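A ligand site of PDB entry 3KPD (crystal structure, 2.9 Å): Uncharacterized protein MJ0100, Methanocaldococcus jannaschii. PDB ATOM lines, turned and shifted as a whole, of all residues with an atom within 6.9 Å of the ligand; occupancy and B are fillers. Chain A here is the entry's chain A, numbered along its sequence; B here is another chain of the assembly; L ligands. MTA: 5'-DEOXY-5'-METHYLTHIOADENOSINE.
An oxygen (O2') of the ligand lies within hydrogen-bond range of the side-chain hydroxyl of Ser 8 (2.5 Å). O2' of the ligand is in hydrogen-bond range of OG1 of Thr 110, at 3.2 Å. An oxygen (O3') of the ligand sits at hydrogen-bond distance from the side-chain carboxylate (OD1) of Asp 113 (2.7 Å). N6 of the ligand sits at hydrogen-bond distance from O of Ile 12 (3.0 Å). The backbone carbonyl oxygen (O) of His 34 sits at hydrogen-bond distance from a nitrogen (N6) of the ligand, 2.8 Å away. N of Ile 12 lies within hydrogen-bond range of N1 of the ligand, 2.8 Å away.
The backbone NH (N) of Ser 8 sits at hydrogen-bond distance from the backbone carbonyl oxygen (O) of Ile 108 (2.8 Å). N of Ile 32 lies within hydrogen-bond range of O of Leu 27 (2.9 Å). The backbone NH (N) of Thr 110 sits at hydrogen-bond distance from the side-chain carboxylate (OD2) of Asp 113, 2.7 Å away. OE2 of Glu 112 sits at hydrogen-bond distance from OG of Ser 111, at 3.3 Å.
Merely in contact with the ligand: Glu 112, Ile 108, Pro 36, Ile 32, Asn 31, Pro 10 and Pro 11. Hydrophobic or aromatic side chains within 4 Å of the ligand: Ile 12, Ile 32, His 34, Pro 36 and Ile 108. Of the 25 residues printed, 12 come within 4 Å of the ligand. The nearest printed residue that does not touch the ligand is Leu 35 (4.4 Å).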
ATOM      1  N   ILE A   6     -11.432  10.713  16.731  1.00  0.00           N
ATOM      2  CA  ILE A   6     -11.512  11.990  17.412  1.00  0.00           C
ATOM      3  C   ILE A   6     -11.599  11.703  18.907  1.00  0.00           C
ATOM      4  O   ILE A   6     -11.041  12.453  19.719  1.00  0.00           O
ATOM      5  CB  ILE A   6     -12.751  12.802  16.905  1.00  0.00           C
ATOM      6  CG1 ILE A   6     -12.355  13.633  15.686  1.00  0.00           C
ATOM      7  CG2 ILE A   6     -13.310  13.734  17.947  1.00  0.00           C
ATOM      8  CD1 ILE A   6     -12.404  12.865  14.336  1.00  0.00           C
ATOM      9  N   LEU A   7     -12.269  10.606  19.252  1.00  0.00           N
ATOM     10  CA  LEU A   7     -12.575  10.249  20.627  1.00  0.00           C
ATOM     11  C   LEU A   7     -11.347  10.158  21.557  1.00  0.00           C
ATOM     12  O   LEU A   7     -10.232   9.895  21.117  1.00  0.00           O
ATOM     13  CB  LEU A   7     -13.396   8.953  20.690  1.00  0.00           C
ATOM     14  CG  LEU A   7     -12.891   7.639  20.083  1.00  0.00           C
ATOM     15  CD1 LEU A   7     -11.987   6.895  21.000  1.00  0.00           C
ATOM     16  CD2 LEU A   7     -14.061   6.751  19.759  1.00  0.00           C
ATOM     17  N   SER A   8     -11.604  10.400  22.848  1.00  0.00           N
ATOM     18  CA  SER A   8     -10.624  10.263  23.917  1.00  0.00           C
ATOM     19  C   SER A   8     -10.411   8.806  24.319  1.00  0.00           C
ATOM     20  O   SER A   8     -11.332   8.063  24.682  1.00  0.00           O
ATOM     21  CB  SER A   8     -10.956  11.168  25.101  1.00  0.00           C
ATOM     22  OG  SER A   8     -10.834  12.520  24.720  1.00  0.00           O
ATOM     23  N   LYS A   9      -9.149   8.436  24.333  1.00  0.00           N
ATOM     24  CA  LYS A   9      -8.726   7.232  23.669  1.00  0.00           C
ATOM     25  C   LYS A   9      -8.652   5.944  24.425  1.00  0.00           C
ATOM     26  O   LYS A   9      -8.962   4.895  23.831  1.00  0.00           O
ATOM     27  CB  LYS A   9      -7.459   7.529  22.879  1.00  0.00           C
ATOM     28  CG  LYS A   9      -7.820   8.275  21.612  1.00  0.00           C
ATOM     29  CD  LYS A   9      -7.040   9.530  21.408  1.00  0.00           C
ATOM     30  CE  LYS A   9      -7.016   9.826  19.916  1.00  0.00           C
ATOM     31  NZ  LYS A   9      -5.587   9.842  19.474  1.00  0.00           N
ATOM     32  N   PRO A  10      -8.176   5.982  25.686  1.00  0.00           N
ATOM     33  CA  PRO A  10      -8.640   4.989  26.670  1.00  0.00           C
ATOM     34  C   PRO A  10      -9.684   5.645  27.586  1.00  0.00           C
ATOM     35  O   PRO A  10      -9.427   6.708  28.164  1.00  0.00           O
ATOM     36  CB  PRO A  10      -7.359   4.630  27.441  1.00  0.00           C
ATOM     37  CG  PRO A  10      -6.388   5.742  27.153  1.00  0.00           C
ATOM     38  CD  PRO A  10      -6.989   6.714  26.172  1.00  0.00           C
ATOM     39  N   PRO A  11     -10.884   5.042  27.709  1.00  0.00           N
ATOM     40  CA  PRO A  11     -11.897   5.700  28.543  1.00  0.00           C
ATOM     41  C   PRO A  11     -11.584   5.615  30.039  1.00  0.00           C
ATOM     42  O   PRO A  11     -10.948   4.659  30.481  1.00  0.00           O
ATOM     43  CB  PRO A  11     -13.182   4.936  28.217  1.00  0.00           C
ATOM     44  CG  PRO A  11     -12.725   3.594  27.748  1.00  0.00           C
ATOM     45  CD  PRO A  11     -11.394   3.819  27.065  1.00  0.00           C
ATOM     46  N   ILE A  12     -12.013   6.631  30.799  1.00  0.00           N
ATOM     47  CA  ILE A  12     -11.992   6.532  32.238  1.00  0.00           C
ATOM     48  C   ILE A  12     -13.410   6.244  32.696  1.00  0.00           C
ATOM     49  O   ILE A  12     -14.331   7.029  32.461  1.00  0.00           O
ATOM     50  CB  ILE A  12     -11.523   7.805  32.955  1.00  0.00           C
ATOM     51  CG1 ILE A  12     -10.269   8.370  32.312  1.00  0.00           C
ATOM     52  CG2 ILE A  12     -11.263   7.518  34.421  1.00  0.00           C
ATOM     53  CD1 ILE A  12      -9.964   9.777  32.785  1.00  0.00           C
ATOM     54  N   THR A  13     -13.577   5.108  33.347  1.00  0.00           N
ATOM     55  CA  THR A  13     -14.872   4.711  33.840  1.00  0.00           C
ATOM     56  C   THR A  13     -14.770   4.402  35.316  1.00  0.00           C
ATOM     57  O   THR A  13     -13.692   4.474  35.926  1.00  0.00           O
ATOM     58  CB  THR A  13     -15.429   3.528  33.062  1.00  0.00           C
ATOM     59  OG1 THR A  13     -14.394   2.553  32.867  1.00  0.00           O
ATOM     60  CG2 THR A  13     -15.905   3.979  31.707  1.00  0.00           C
ATOM     61  N   LEU A  27     -13.022  13.175  38.458  1.00  0.00           N
ATOM     62  CA  LEU A  27     -13.257  14.301  37.530  1.00  0.00           C
ATOM     63  C   LEU A  27     -12.171  15.374  37.638  1.00  0.00           C
ATOM     64  O   LEU A  27     -11.568  15.750  36.648  1.00  0.00           O
ATOM     65  CB  LEU A  27     -14.617  14.951  37.779  1.00  0.00           C
ATOM     66  CG  LEU A  27     -15.950  14.215  37.623  1.00  0.00           C
ATOM     67  CD1 LEU A  27     -17.066  15.184  37.819  1.00  0.00           C
ATOM     68  CD2 LEU A  27     -16.107  13.531  36.273  1.00  0.00           C
ATOM     69  N   HIS A  30      -8.399  14.161  36.404  1.00  0.00           N
ATOM     70  CA  HIS A  30      -8.064  14.054  34.986  1.00  0.00           C
ATOM     71  C   HIS A  30      -8.492  15.274  34.225  1.00  0.00           C
ATOM     72  O   HIS A  30      -8.180  15.428  33.033  1.00  0.00           O
ATOM     73  CB  HIS A  30      -8.670  12.791  34.397  1.00  0.00           C
ATOM     74  CG  HIS A  30      -8.255  11.537  35.110  1.00  0.00           C
ATOM     75  ND1 HIS A  30      -8.869  11.104  36.263  1.00  0.00           N
ATOM     76  CD2 HIS A  30      -7.267  10.651  34.843  1.00  0.00           C
ATOM     77  CE1 HIS A  30      -8.284   9.988  36.674  1.00  0.00           C
ATOM     78  NE2 HIS A  30      -7.309   9.690  35.822  1.00  0.00           N
ATOM     79  N   ASN A  31      -9.184  16.178  34.927  1.00  0.00           N
ATOM     80  CA  ASN A  31      -9.658  17.416  34.334  1.00  0.00           C
ATOM     81  C   ASN A  31     -10.825  17.141  33.369  1.00  0.00           C
ATOM     82  O   ASN A  31     -10.912  17.723  32.296  1.00  0.00           O
ATOM     83  CB  ASN A  31      -8.509  18.163  33.620  1.00  0.00           C
ATOM     84  CG  ASN A  31      -8.863  19.601  33.330  1.00  0.00           C
ATOM     85  OD1 ASN A  31      -9.625  20.234  34.071  1.00  0.00           O
ATOM     86  ND2 ASN A  31      -8.317  20.124  32.228  1.00  0.00           N
ATOM     87  N   ILE A  32     -11.710  16.258  33.784  1.00  0.00           N
ATOM     88  CA  ILE A  32     -12.804  15.807  32.935  1.00  0.00           C
ATOM     89  C   ILE A  32     -14.168  16.191  33.508  1.00  0.00           C
ATOM     90  O   ILE A  32     -14.276  16.462  34.699  1.00  0.00           O
ATOM     91  CB  ILE A  32     -12.733  14.284  32.724  1.00  0.00           C
ATOM     92  CG1 ILE A  32     -12.705  13.569  34.079  1.00  0.00           C
ATOM     93  CG2 ILE A  32     -11.480  13.914  31.881  1.00  0.00           C
ATOM     94  CD1 ILE A  32     -13.401  12.212  34.055  1.00  0.00           C
ATOM     95  N   ASN A  33     -15.196  16.247  32.679  1.00  0.00           N
ATOM     96  CA  ASN A  33     -16.533  16.491  33.202  1.00  0.00           C
ATOM     97  C   ASN A  33     -17.500  15.334  33.012  1.00  0.00           C
ATOM     98  O   ASN A  33     -18.683  15.483  33.287  1.00  0.00           O
ATOM     99  CB  ASN A  33     -17.118  17.774  32.642  1.00  0.00           C
ATOM    100  CG  ASN A  33     -18.347  18.235  33.421  1.00  0.00           C
ATOM    101  OD1 ASN A  33     -18.419  18.051  34.631  1.00  0.00           O
ATOM    102  ND2 ASN A  33     -19.297  18.829  32.730  1.00  0.00           N
ATOM    103  N   HIS A  34     -17.008  14.181  32.570  1.00  0.00           N
ATOM    104  CA  HIS A  34     -17.891  13.077  32.204  1.00  0.00           C
ATOM    105  C   HIS A  34     -17.337  11.798  32.716  1.00  0.00           C
ATOM    106  O   HIS A  34     -16.213  11.431  32.387  1.00  0.00           O
ATOM    107  CB  HIS A  34     -18.068  12.984  30.690  1.00  0.00           C
ATOM    108  CG  HIS A  34     -18.803  14.148  30.109  1.00  0.00           C
ATOM    109  ND1 HIS A  34     -18.162  15.296  29.693  1.00  0.00           N
ATOM    110  CD2 HIS A  34     -20.124  14.359  29.911  1.00  0.00           C
ATOM    111  CE1 HIS A  34     -19.064  16.149  29.247  1.00  0.00           C
ATOM    112  NE2 HIS A  34     -20.255  15.610  29.373  1.00  0.00           N
ATOM    113  N   LEU A  35     -18.120  11.101  33.533  1.00  0.00           N
ATOM    114  CA  LEU A  35     -17.670   9.831  34.059  1.00  0.00           C
ATOM    115  C   LEU A  35     -18.696   8.783  33.739  1.00  0.00           C
ATOM    116  O   LEU A  35     -19.773   8.783  34.329  1.00  0.00           O
ATOM    117  CB  LEU A  35     -17.399   9.911  35.569  1.00  0.00           C
ATOM    118  CG  LEU A  35     -16.666   8.703  36.161  1.00  0.00           C
ATOM    119  CD1 LEU A  35     -15.308   8.466  35.475  1.00  0.00           C
ATOM    120  CD2 LEU A  35     -16.476   8.884  37.663  1.00  0.00           C
ATOM    121  N   PRO A  36     -18.371   7.893  32.773  1.00  0.00           N
ATOM    122  CA  PRO A  36     -19.218   6.758  32.492  1.00  0.00           C
ATOM    123  C   PRO A  36     -19.118   5.733  33.608  1.00  0.00           C
ATOM    124  O   PRO A  36     -18.033   5.356  34.034  1.00  0.00           O
ATOM    125  CB  PRO A  36     -18.645   6.197  31.179  1.00  0.00           C
ATOM    126  CG  PRO A  36     -17.825   7.264  30.620  1.00  0.00           C
ATOM    127  CD  PRO A  36     -17.284   8.029  31.793  1.00  0.00           C
ATOM    128  N   GLY A 107     -14.618   4.618  24.371  1.00  0.00           N
ATOM    129  CA  GLY A 107     -14.119   5.991  24.434  1.00  0.00           C
ATOM    130  C   GLY A 107     -15.139   7.036  24.806  1.00  0.00           C
ATOM    131  O   GLY A 107     -16.207   6.728  25.333  1.00  0.00           O
ATOM    132  N   ILE A 108     -14.823   8.274  24.499  1.00  0.00           N
ATOM    133  CA  ILE A 108     -15.713   9.394  24.782  1.00  0.00           C
ATOM    134  C   ILE A 108     -15.387  10.569  23.890  1.00  0.00           C
ATOM    135  O   ILE A 108     -14.224  10.838  23.638  1.00  0.00           O
ATOM    136  CB  ILE A 108     -15.596   9.797  26.249  1.00  0.00           C
ATOM    137  CG1 ILE A 108     -16.602  10.880  26.598  1.00  0.00           C
ATOM    138  CG2 ILE A 108     -14.209  10.295  26.549  1.00  0.00           C
ATOM    139  CD1 ILE A 108     -16.902  10.905  28.091  1.00  0.00           C
ATOM    140  N   VAL A 109     -16.415  11.233  23.388  1.00  0.00           N
ATOM    141  CA  VAL A 109     -16.257  12.479  22.648  1.00  0.00           C
ATOM    142  C   VAL A 109     -16.896  13.579  23.460  1.00  0.00           C
ATOM    143  O   VAL A 109     -17.995  13.435  23.970  1.00  0.00           O
ATOM    144  CB  VAL A 109     -16.952  12.479  21.257  1.00  0.00           C
ATOM    145  CG1 VAL A 109     -16.728  13.803  20.551  1.00  0.00           C
ATOM    146  CG2 VAL A 109     -16.432  11.369  20.384  1.00  0.00           C
ATOM    147  N   THR A 110     -16.206  14.697  23.578  1.00  0.00           N
ATOM    148  CA  THR A 110     -16.800  15.896  24.155  1.00  0.00           C
ATOM    149  C   THR A 110     -16.782  16.989  23.121  1.00  0.00           C
ATOM    150  O   THR A 110     -15.969  16.954  22.205  1.00  0.00           O
ATOM    151  CB  THR A 110     -16.034  16.333  25.367  1.00  0.00           C
ATOM    152  OG1 THR A 110     -14.666  16.499  24.998  1.00  0.00           O
ATOM    153  CG2 THR A 110     -16.110  15.275  26.430  1.00  0.00           C
ATOM    154  N   SER A 111     -17.674  17.964  23.252  1.00  0.00           N
ATOM    155  CA  SER A 111     -17.656  19.150  22.370  1.00  0.00           C
ATOM    156  C   SER A 111     -16.256  19.766  22.367  1.00  0.00           C
ATOM    157  O   SER A 111     -15.776  20.249  21.350  1.00  0.00           O
ATOM    158  CB  SER A 111     -18.750  20.158  22.747  1.00  0.00           C
ATOM    159  OG  SER A 111     -18.884  20.285  24.154  1.00  0.00           O
ATOM    160  N   GLU A 112     -15.606  19.691  23.529  1.00  0.00           N
ATOM    161  CA  GLU A 112     -14.198  20.039  23.676  1.00  0.00           C
ATOM    162  C   GLU A 112     -13.310  19.470  22.546  1.00  0.00           C
ATOM    163  O   GLU A 112     -12.361  20.123  22.144  1.00  0.00           O
ATOM    164  CB  GLU A 112     -13.682  19.592  25.051  1.00  0.00           C
ATOM    165  CG  GLU A 112     -14.217  20.388  26.269  1.00  0.00           C
ATOM    166  CD  GLU A 112     -15.452  19.772  26.972  1.00  0.00           C
ATOM    167  OE1 GLU A 112     -15.317  19.203  28.078  1.00  0.00           O
ATOM    168  OE2 GLU A 112     -16.575  19.876  26.420  1.00  0.00           O
ATOM    169  N   ASP A 113     -13.634  18.276  22.036  1.00  0.00           N
ATOM    170  CA  ASP A 113     -12.887  17.642  20.938  1.00  0.00           C
ATOM    171  C   ASP A 113     -13.426  18.100  19.585  1.00  0.00           C
ATOM    172  O   ASP A 113     -12.659  18.408  18.679  1.00  0.00           O
ATOM    173  CB  ASP A 113     -12.969  16.100  21.024  1.00  0.00           C
ATOM    174  CG  ASP A 113     -12.731  15.558  22.448  1.00  0.00           C
ATOM    175  OD1 ASP A 113     -11.630  15.780  23.006  1.00  0.00           O
ATOM    176  OD2 ASP A 113     -13.625  14.874  22.996  1.00  0.00           O
ATOM    177  N   ARG A 116     -12.178  21.292  17.467  1.00  0.00           N
ATOM    178  CA  ARG A 116     -10.805  21.285  16.940  1.00  0.00           C
ATOM    179  C   ARG A 116     -11.034  20.877  15.495  1.00  0.00           C
ATOM    180  O   ARG A 116     -10.106  20.767  14.693  1.00  0.00           O
ATOM    181  CB  ARG A 116      -9.899  20.332  17.713  1.00  0.00           C
ATOM    182  CG  ARG A 116      -9.656  20.771  19.174  1.00  0.00           C
ATOM    183  CD  ARG A 116      -8.263  20.373  19.689  1.00  0.00           C
ATOM    184  NE  ARG A 116      -7.995  20.905  21.026  1.00  0.00           N
ATOM    185  CZ  ARG A 116      -7.757  20.173  22.116  1.00  0.00           C
ATOM    186  NH1 ARG A 116      -7.734  18.837  22.058  1.00  0.00           N
ATOM    187  NH2 ARG A 116      -7.531  20.773  23.284  1.00  0.00           N
ATOM    188  N   ASN B  92     -13.451  26.987  25.808  1.00  0.00           N
ATOM    189  CA  ASN B  92     -14.135  25.795  26.297  1.00  0.00           C
ATOM    190  C   ASN B  92     -14.945  26.007  27.566  1.00  0.00           C
ATOM    191  O   ASN B  92     -14.624  25.480  28.645  1.00  0.00           O
ATOM    192  CB  ASN B  92     -13.210  24.582  26.342  1.00  0.00           C
ATOM    193  CG  ASN B  92     -13.372  23.705  25.116  1.00  0.00           C
ATOM    194  OD1 ASN B  92     -12.396  23.388  24.404  1.00  0.00           O
ATOM    195  ND2 ASN B  92     -14.627  23.314  24.824  1.00  0.00           N
HETATM  196  CS  MTA L   1     -12.827  17.774  29.222  1.00  0.00           C
HETATM  197  S5' MTA L   1     -11.571  18.260  28.063  1.00  0.00           S
HETATM  198  C5' MTA L   1     -10.160  17.206  28.302  1.00  0.00           C
HETATM  199  C4' MTA L   1     -10.334  15.822  27.646  1.00  0.00           C
HETATM  200  O4' MTA L   1     -10.921  14.842  28.503  1.00  0.00           O
HETATM  201  C2' MTA L   1     -12.295  14.805  26.653  1.00  0.00           C
HETATM  202  O2' MTA L   1     -12.665  14.051  25.488  1.00  0.00           O
HETATM  203  C3' MTA L   1     -11.194  15.823  26.393  1.00  0.00           C
HETATM  204  O3' MTA L   1     -10.297  15.411  25.367  1.00  0.00           O
HETATM  205  C1' MTA L   1     -11.641  13.927  27.682  1.00  0.00           C
HETATM  206  N9  MTA L   1     -12.549  13.136  28.535  1.00  0.00           N
HETATM  207  C8  MTA L   1     -13.657  13.555  29.180  1.00  0.00           C
HETATM  208  N7  MTA L   1     -14.228  12.557  29.890  1.00  0.00           N
HETATM  209  C5  MTA L   1     -13.467  11.470  29.730  1.00  0.00           C
HETATM  210  C6  MTA L   1     -13.482  10.079  30.202  1.00  0.00           C
HETATM  211  N6  MTA L   1     -14.460   9.653  31.029  1.00  0.00           N
HETATM  212  N1  MTA L   1     -12.493   9.252  29.804  1.00  0.00           N
HETATM  213  C2  MTA L   1     -11.503   9.668  28.985  1.00  0.00           C
HETATM  214  N3  MTA L   1     -11.423  10.928  28.504  1.00  0.00           N
HETATM  215  C4  MTA L   1     -12.350  11.862  28.842  1.00  0.00           C
